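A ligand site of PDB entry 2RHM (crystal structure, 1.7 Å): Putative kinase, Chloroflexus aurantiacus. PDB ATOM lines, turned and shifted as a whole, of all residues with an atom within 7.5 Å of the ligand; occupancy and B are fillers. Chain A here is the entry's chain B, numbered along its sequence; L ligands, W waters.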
ATOM      1  N   HIS A  13      -9.662 -31.034  -5.646  1.00  0.00           N
ATOM      2  CA  HIS A  13      -8.366 -31.477  -5.174  1.00  0.00           C
ATOM      3  C   HIS A  13      -7.420 -30.262  -4.958  1.00  0.00           C
ATOM      4  O   HIS A  13      -7.662 -29.183  -5.473  1.00  0.00           O
ATOM      5  CB  HIS A  13      -7.741 -32.474  -6.138  1.00  0.00           C
ATOM      6  CG  HIS A  13      -8.357 -33.827  -6.073  1.00  0.00           C
ATOM      7  ND1 HIS A  13      -8.529 -34.506  -4.893  1.00  0.00           N
ATOM      8  CD2 HIS A  13      -8.807 -34.657  -7.055  1.00  0.00           C
ATOM      9  CE1 HIS A  13      -9.055 -35.694  -5.140  1.00  0.00           C
ATOM     10  NE2 HIS A  13      -9.229 -35.809  -6.445  1.00  0.00           N
ATOM     11  N   PRO A  14      -6.356 -30.440  -4.154  1.00  0.00           N
ATOM     12  CA  PRO A  14      -5.396 -29.349  -4.009  1.00  0.00           C
ATOM     13  C   PRO A  14      -4.864 -28.820  -5.363  1.00  0.00           C
ATOM     14  O   PRO A  14      -4.605 -29.579  -6.298  1.00  0.00           O
ATOM     15  CB  PRO A  14      -4.283 -30.003  -3.189  1.00  0.00           C
ATOM     16  CG  PRO A  14      -5.045 -31.008  -2.331  1.00  0.00           C
ATOM     17  CD  PRO A  14      -6.018 -31.587  -3.303  1.00  0.00           C
ATOM     18  N   ALA A  15      -4.786 -27.491  -5.446  1.00  0.00           N
ATOM     19  CA  ALA A  15      -4.287 -26.774  -6.626  1.00  0.00           C
ATOM     20  C   ALA A  15      -5.262 -26.682  -7.816  1.00  0.00           C
ATOM     21  O   ALA A  15      -4.894 -26.193  -8.875  1.00  0.00           O
ATOM     22  CB  ALA A  15      -2.905 -27.296  -7.071  1.00  0.00           C
ATOM     23  N   THR A  16      -6.513 -27.113  -7.648  1.00  0.00           N
ATOM     24  CA  THR A  16      -7.494 -27.028  -8.743  1.00  0.00           C
ATOM     25  C   THR A  16      -8.107 -25.635  -8.981  1.00  0.00           C
ATOM     26  O   THR A  16      -8.945 -25.489  -9.881  1.00  0.00           O
ATOM     27  CB  THR A  16      -8.656 -28.011  -8.516  1.00  0.00           C
ATOM     28  OG1 THR A  16      -9.221 -27.812  -7.211  1.00  0.00           O
ATOM     29  CG2 THR A  16      -8.189 -29.456  -8.674  1.00  0.00           C
ATOM     30  N   GLY A  17      -7.742 -24.650  -8.165  1.00  0.00           N
ATOM     31  CA  GLY A  17      -8.267 -23.293  -8.286  1.00  0.00           C
ATOM     32  C   GLY A  17      -9.325 -22.938  -7.258  1.00  0.00           C
ATOM     33  O   GLY A  17      -9.846 -21.809  -7.247  1.00  0.00           O
ATOM     34  N   LYS A  18      -9.669 -23.879  -6.393  1.00  0.00           N
ATOM     35  CA  LYS A  18     -10.698 -23.630  -5.380  1.00  0.00           C
ATOM     36  C   LYS A  18     -10.393 -22.457  -4.457  1.00  0.00           C
ATOM     37  O   LYS A  18     -11.305 -21.747  -4.019  1.00  0.00           O
ATOM     38  CB  LYS A  18     -11.002 -24.916  -4.587  1.00  0.00           C
ATOM     39  CG  LYS A  18      -9.825 -25.488  -3.829  1.00  0.00           C
ATOM     40  CD  LYS A  18     -10.263 -26.753  -3.038  1.00  0.00           C
ATOM     41  CE  LYS A  18      -9.091 -27.461  -2.406  1.00  0.00           C
ATOM     42  NZ  LYS A  18      -8.288 -26.599  -1.523  1.00  0.00           N
ATOM     43  N   THR A  19      -9.122 -22.214  -4.161  1.00  0.00           N
ATOM     44  CA  THR A  19      -8.802 -21.092  -3.289  1.00  0.00           C
ATOM     45  C   THR A  19      -9.161 -19.772  -3.977  1.00  0.00           C
ATOM     46  O   THR A  19      -9.927 -18.959  -3.463  1.00  0.00           O
ATOM     47  CB  THR A  19      -7.315 -21.067  -2.921  1.00  0.00           C
ATOM     48  OG1 THR A  19      -6.966 -22.310  -2.332  1.00  0.00           O
ATOM     49  CG2 THR A  19      -7.057 -19.952  -1.966  1.00  0.00           C
ATOM     50  N   ASP A  37      -7.575 -24.622   4.695  1.00  0.00           N
ATOM     51  CA  ASP A  37      -6.148 -24.287   4.689  1.00  0.00           C
ATOM     52  C   ASP A  37      -5.860 -22.968   5.410  1.00  0.00           C
ATOM     53  O   ASP A  37      -4.832 -22.870   6.108  1.00  0.00           O
ATOM     54  CB  ASP A  37      -5.588 -24.317   3.276  1.00  0.00           C
ATOM     55  CG  ASP A  37      -5.241 -25.738   2.796  1.00  0.00           C
ATOM     56  OD1 ASP A  37      -5.307 -26.724   3.570  1.00  0.00           O
ATOM     57  OD2 ASP A  37      -4.875 -25.866   1.621  1.00  0.00           O
ATOM     58  N   GLU A  83     -14.706 -23.718   1.939  1.00  0.00           N
ATOM     59  CA  GLU A  83     -13.782 -24.234   0.945  1.00  0.00           C
ATOM     60  C   GLU A  83     -12.812 -25.232   1.561  1.00  0.00           C
ATOM     61  O   GLU A  83     -12.166 -24.939   2.577  1.00  0.00           O
ATOM     62  CB  GLU A  83     -13.011 -23.072   0.300  1.00  0.00           C
ATOM     63  CG  GLU A  83     -11.954 -23.534  -0.686  1.00  0.00           C
ATOM     64  CD  GLU A  83     -10.589 -23.771  -0.028  1.00  0.00           C
ATOM     65  OE1 GLU A  83     -10.016 -22.830   0.587  1.00  0.00           O
ATOM     66  OE2 GLU A  83     -10.067 -24.895  -0.126  1.00  0.00           O
ATOM     67  N   LEU A 118      -1.888 -29.587 -12.504  1.00  0.00           N
ATOM     68  CA  LEU A 118      -1.857 -29.665 -11.059  1.00  0.00           C
ATOM     69  C   LEU A 118      -0.423 -29.868 -10.570  1.00  0.00           C
ATOM     70  O   LEU A 118      -0.004 -29.249  -9.586  1.00  0.00           O
ATOM     71  CB  LEU A 118      -2.781 -30.792 -10.549  1.00  0.00           C
ATOM     72  CG  LEU A 118      -4.296 -30.579 -10.769  1.00  0.00           C
ATOM     73  CD1 LEU A 118      -5.113 -31.771 -10.255  1.00  0.00           C
ATOM     74  CD2 LEU A 118      -4.765 -29.315 -10.106  1.00  0.00           C
ATOM     75  N   ARG A 121       1.530 -26.584 -10.708  1.00  0.00           N
ATOM     76  CA  ARG A 121       1.116 -25.654  -9.672  1.00  0.00           C
ATOM     77  C   ARG A 121       1.634 -26.031  -8.306  1.00  0.00           C
ATOM     78  O   ARG A 121       2.137 -25.172  -7.570  1.00  0.00           O
ATOM     79  CB  ARG A 121      -0.417 -25.584  -9.598  1.00  0.00           C
ATOM     80  CG  ARG A 121      -1.033 -24.878 -10.745  1.00  0.00           C
ATOM     81  CD  ARG A 121      -2.546 -24.949 -10.693  1.00  0.00           C
ATOM     82  NE  ARG A 121      -3.091 -24.315 -11.888  1.00  0.00           N
ATOM     83  CZ  ARG A 121      -4.351 -24.405 -12.289  1.00  0.00           C
ATOM     84  NH1 ARG A 121      -5.246 -25.091 -11.582  1.00  0.00           N
ATOM     85  NH2 ARG A 121      -4.720 -23.787 -13.403  1.00  0.00           N
ATOM     86  N   ILE A 122       1.506 -27.301  -7.963  1.00  0.00           N
ATOM     87  CA  ILE A 122       1.982 -27.783  -6.670  1.00  0.00           C
ATOM     88  C   ILE A 122       3.456 -27.445  -6.505  1.00  0.00           C
ATOM     89  O   ILE A 122       3.866 -26.867  -5.493  1.00  0.00           O
ATOM     90  CB  ILE A 122       1.745 -29.305  -6.545  1.00  0.00           C
ATOM     91  CG1 ILE A 122       0.259 -29.571  -6.306  1.00  0.00           C
ATOM     92  CG2 ILE A 122       2.550 -29.890  -5.387  1.00  0.00           C
ATOM     93  CD1 ILE A 122      -0.105 -31.013  -6.330  1.00  0.00           C
ATOM     94  N   LEU A 123       4.240 -27.762  -7.529  1.00  0.00           N
ATOM     95  CA  LEU A 123       5.676 -27.526  -7.509  1.00  0.00           C
ATOM     96  C   LEU A 123       6.054 -26.049  -7.397  1.00  0.00           C
ATOM     97  O   LEU A 123       6.852 -25.679  -6.540  1.00  0.00           O
ATOM     98  CB  LEU A 123       6.333 -28.137  -8.743  1.00  0.00           C
ATOM     99  CG  LEU A 123       6.399 -29.667  -8.804  1.00  0.00           C
ATOM    100  CD1 LEU A 123       6.920 -30.117 -10.159  1.00  0.00           C
ATOM    101  CD2 LEU A 123       7.271 -30.218  -7.678  1.00  0.00           C
ATOM    102  N   SER A 124       5.472 -25.221  -8.266  1.00  0.00           N
ATOM    103  CA  SER A 124       5.769 -23.792  -8.266  1.00  0.00           C
ATOM    104  C   SER A 124       5.328 -23.101  -6.971  1.00  0.00           C
ATOM    105  O   SER A 124       6.044 -22.237  -6.461  1.00  0.00           O
ATOM    106  CB  SER A 124       5.130 -23.108  -9.475  1.00  0.00           C
ATOM    107  OG  SER A 124       3.719 -23.160  -9.412  1.00  0.00           O
ATOM    108  N   ARG A 125       4.164 -23.466  -6.439  1.00  0.00           N
ATOM    109  CA  ARG A 125       3.670 -22.866  -5.193  1.00  0.00           C
ATOM    110  C   ARG A 125       4.586 -23.166  -4.017  1.00  0.00           C
ATOM    111  O   ARG A 125       4.792 -22.320  -3.161  1.00  0.00           O
ATOM    112  CB  ARG A 125       2.239 -23.326  -4.900  1.00  0.00           C
ATOM    113  CG  ARG A 125       1.237 -22.682  -5.844  1.00  0.00           C
ATOM    114  CD  ARG A 125      -0.166 -23.273  -5.755  1.00  0.00           C
ATOM    115  NE  ARG A 125      -0.990 -22.709  -6.832  1.00  0.00           N
ATOM    116  CZ  ARG A 125      -2.308 -22.857  -6.953  1.00  0.00           C
ATOM    117  NH1 ARG A 125      -3.011 -23.546  -6.072  1.00  0.00           N
ATOM    118  NH2 ARG A 125      -2.922 -22.290  -7.982  1.00  0.00           N
ATOM    119  N   ILE A 126       5.135 -24.378  -3.983  1.00  0.00           N
ATOM    120  CA  ILE A 126       6.059 -24.787  -2.926  1.00  0.00           C
ATOM    121  C   ILE A 126       7.425 -24.137  -3.139  1.00  0.00           C
ATOM    122  O   ILE A 126       8.075 -23.714  -2.178  1.00  0.00           O
ATOM    123  CB  ILE A 126       6.170 -26.333  -2.838  1.00  0.00           C
ATOM    124  CG1 ILE A 126       4.852 -26.915  -2.310  1.00  0.00           C
ATOM    125  CG2 ILE A 126       7.333 -26.737  -1.941  1.00  0.00           C
ATOM    126  CD1 ILE A 126       4.779 -28.427  -2.366  1.00  0.00           C
ATOM    127  N   ALA A 130       4.518 -19.595  -1.878  1.00  0.00           N
ATOM    128  CA  ALA A 130       3.125 -19.177  -1.765  1.00  0.00           C
ATOM    129  C   ALA A 130       2.410 -20.078  -0.755  1.00  0.00           C
ATOM    130  O   ALA A 130       1.451 -19.665  -0.095  1.00  0.00           O
ATOM    131  CB  ALA A 130       2.448 -19.251  -3.125  1.00  0.00           C
ATOM    132  N   ARG A 131       2.871 -21.316  -0.649  1.00  0.00           N
ATOM    133  CA  ARG A 131       2.323 -22.315   0.249  1.00  0.00           C
ATOM    134  C   ARG A 131       3.013 -22.262   1.634  1.00  0.00           C
ATOM    135  O   ARG A 131       4.239 -22.268   1.730  1.00  0.00           O
ATOM    136  CB  ARG A 131       2.518 -23.670  -0.427  1.00  0.00           C
ATOM    137  CG  ARG A 131       1.843 -24.851   0.183  1.00  0.00           C
ATOM    138  CD  ARG A 131       0.340 -24.743   0.103  1.00  0.00           C
ATOM    139  NE  ARG A 131      -0.275 -25.934   0.659  1.00  0.00           N
ATOM    140  CZ  ARG A 131      -1.568 -26.053   0.896  1.00  0.00           C
ATOM    141  NH1 ARG A 131      -2.386 -25.043   0.664  1.00  0.00           N
ATOM    142  NH2 ARG A 131      -2.027 -27.193   1.398  1.00  0.00           N
ATOM    143  N   HIS A 135       2.278 -27.082   6.020  1.00  0.00           N
ATOM    144  CA  HIS A 135       1.390 -28.035   5.347  1.00  0.00           C
ATOM    145  C   HIS A 135       2.119 -29.325   5.046  1.00  0.00           C
ATOM    146  O   HIS A 135       1.507 -30.407   5.004  1.00  0.00           O
ATOM    147  CB  HIS A 135       0.820 -27.462   4.058  1.00  0.00           C
ATOM    148  CG  HIS A 135      -0.167 -26.362   4.262  1.00  0.00           C
ATOM    149  ND1 HIS A 135      -1.406 -26.558   4.844  1.00  0.00           N
ATOM    150  CD2 HIS A 135      -0.127 -25.051   3.917  1.00  0.00           C
ATOM    151  CE1 HIS A 135      -2.065 -25.421   4.845  1.00  0.00           C
ATOM    152  NE2 HIS A 135      -1.318 -24.492   4.287  1.00  0.00           N
ATOM    153  N   CYS A 136       3.440 -29.222   4.845  1.00  0.00           N
ATOM    154  CA  CYS A 136       4.269 -30.389   4.586  1.00  0.00           C
ATOM    155  C   CYS A 136       3.640 -31.208   3.479  1.00  0.00           C
ATOM    156  O   CYS A 136       3.407 -32.407   3.645  1.00  0.00           O
ATOM    157  CB  CYS A 136       4.435 -31.225   5.841  1.00  0.00           C
ATOM    158  SG  CYS A 136       5.452 -30.488   7.100  1.00  0.00           S
ATOM    159  N   ASP A 137       3.343 -30.539   2.371  1.00  0.00           N
ATOM    160  CA  ASP A 137       2.685 -31.158   1.243  1.00  0.00           C
ATOM    161  C   ASP A 137       3.535 -32.248   0.625  1.00  0.00           C
ATOM    162  O   ASP A 137       4.685 -32.018   0.280  1.00  0.00           O
ATOM    163  CB  ASP A 137       2.406 -30.127   0.177  1.00  0.00           C
ATOM    164  CG  ASP A 137       1.388 -29.124   0.623  1.00  0.00           C
ATOM    165  OD1 ASP A 137       0.274 -29.537   0.976  1.00  0.00           O
ATOM    166  OD2 ASP A 137       1.729 -27.925   0.603  1.00  0.00           O
ATOM    167  N   ASP A 138       2.931 -33.425   0.509  1.00  0.00           N
ATOM    168  CA  ASP A 138       3.571 -34.556  -0.124  1.00  0.00           C
ATOM    169  C   ASP A 138       3.933 -34.121  -1.540  1.00  0.00           C
ATOM    170  O   ASP A 138       3.050 -33.844  -2.348  1.00  0.00           O
ATOM    171  CB  ASP A 138       2.608 -35.748  -0.124  1.00  0.00           C
ATOM    172  N   ARG A 139       5.248 -34.022  -1.798  1.00  0.00           N
ATOM    173  CA  ARG A 139       5.766 -33.522  -3.071  1.00  0.00           C
ATOM    174  C   ARG A 139       6.814 -34.441  -3.690  1.00  0.00           C
ATOM    175  O   ARG A 139       7.589 -34.011  -4.548  1.00  0.00           O
ATOM    176  CB  ARG A 139       6.399 -32.151  -2.865  1.00  0.00           C
ATOM    177  N   VAL A 147      -0.874 -37.486  -7.937  1.00  0.00           N
ATOM    178  CA  VAL A 147      -1.579 -36.271  -8.324  1.00  0.00           C
ATOM    179  C   VAL A 147      -1.962 -36.304  -9.793  1.00  0.00           C
ATOM    180  O   VAL A 147      -3.092 -35.959 -10.175  1.00  0.00           O
ATOM    181  CB  VAL A 147      -0.706 -35.017  -8.064  1.00  0.00           C
ATOM    182  CG1 VAL A 147      -1.220 -33.801  -8.847  1.00  0.00           C
ATOM    183  CG2 VAL A 147      -0.642 -34.728  -6.565  1.00  0.00           C
HETATM  184  C1  LIG L   1      -2.702 -25.680  -2.787  1.00  0.00           C
HETATM  185  O1  LIG L   1      -2.580 -24.539  -3.291  1.00  0.00           O
HETATM  186  O2  LIG L   1      -3.813 -26.038  -2.293  1.00  0.00           O
HETATM  187  C2  LIG L   1      -1.527 -26.597  -2.751  1.00  0.00           C
HETATM  188  C3  LIG L   1      -0.314 -26.188  -3.295  1.00  0.00           C
HETATM  189  C4  LIG L   1       0.779 -27.040  -3.260  1.00  0.00           C
HETATM  190  C5  LIG L   1       0.651 -28.305  -2.686  1.00  0.00           C
HETATM  191  C6  LIG L   1      -0.569 -28.716  -2.147  1.00  0.00           C
HETATM  192  C7  LIG L   1      -1.663 -27.855  -2.167  1.00  0.00           C
HETATM  193  O   HOH W   1      -6.099 -25.666  -3.389  1.00  0.00           O
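The guanidinium group (NH1) of Arg 131 lies within salt-bridge range of an oxygen (O2) of the ligand (3.4 Å). NH1 of Arg 125 lies within salt-bridge range of O1 of the ligand (3.0 Å).
Water W1 lies within hydrogen-bond range of O2 of the ligand (2.6 Å), NZ of Lys 18 (3.0 Å) and N of Ala 15 (3.0 Å).
The guanidinium group of Arg 131 is in salt-bridge range of the side-chain carboxylate of Asp 37, 2.8 Å away. O of Arg 125 sits at hydrogen-bond distance from N of Arg 131, at 3.3 Å. The guanidinium group of Arg 121 lies within hydrogen-bond range of the backbone carbonyl oxygen of Ala 15. The backbone NH (N) of Ala 130 is in hydrogen-bond range of the backbone carbonyl oxygen (O) of Arg 125 (3.0 Å). The side-chain carboxylate (OD2) of Asp 137 is in salt-bridge range of the guanidinium group (NE) of Arg 131 (2.8 Å).
Merely in contact with the ligand: Asp 137 (3.3 Å), Pro 14 (3.5 Å), Ala 15 (3.6 Å) and Ile 122 (3.7 Å). Hydrophobic or aromatic side chains within 4 Å of the ligand: Pro 14 and Ile 122. Six residues have an atom within 4 Å of the ligand: Pro 14, Ala 15, Ile 122, Arg 125, Arg 131 and Asp 137. The nearest printed residue that does not touch the ligand is Asp 37 (4.1 Å).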
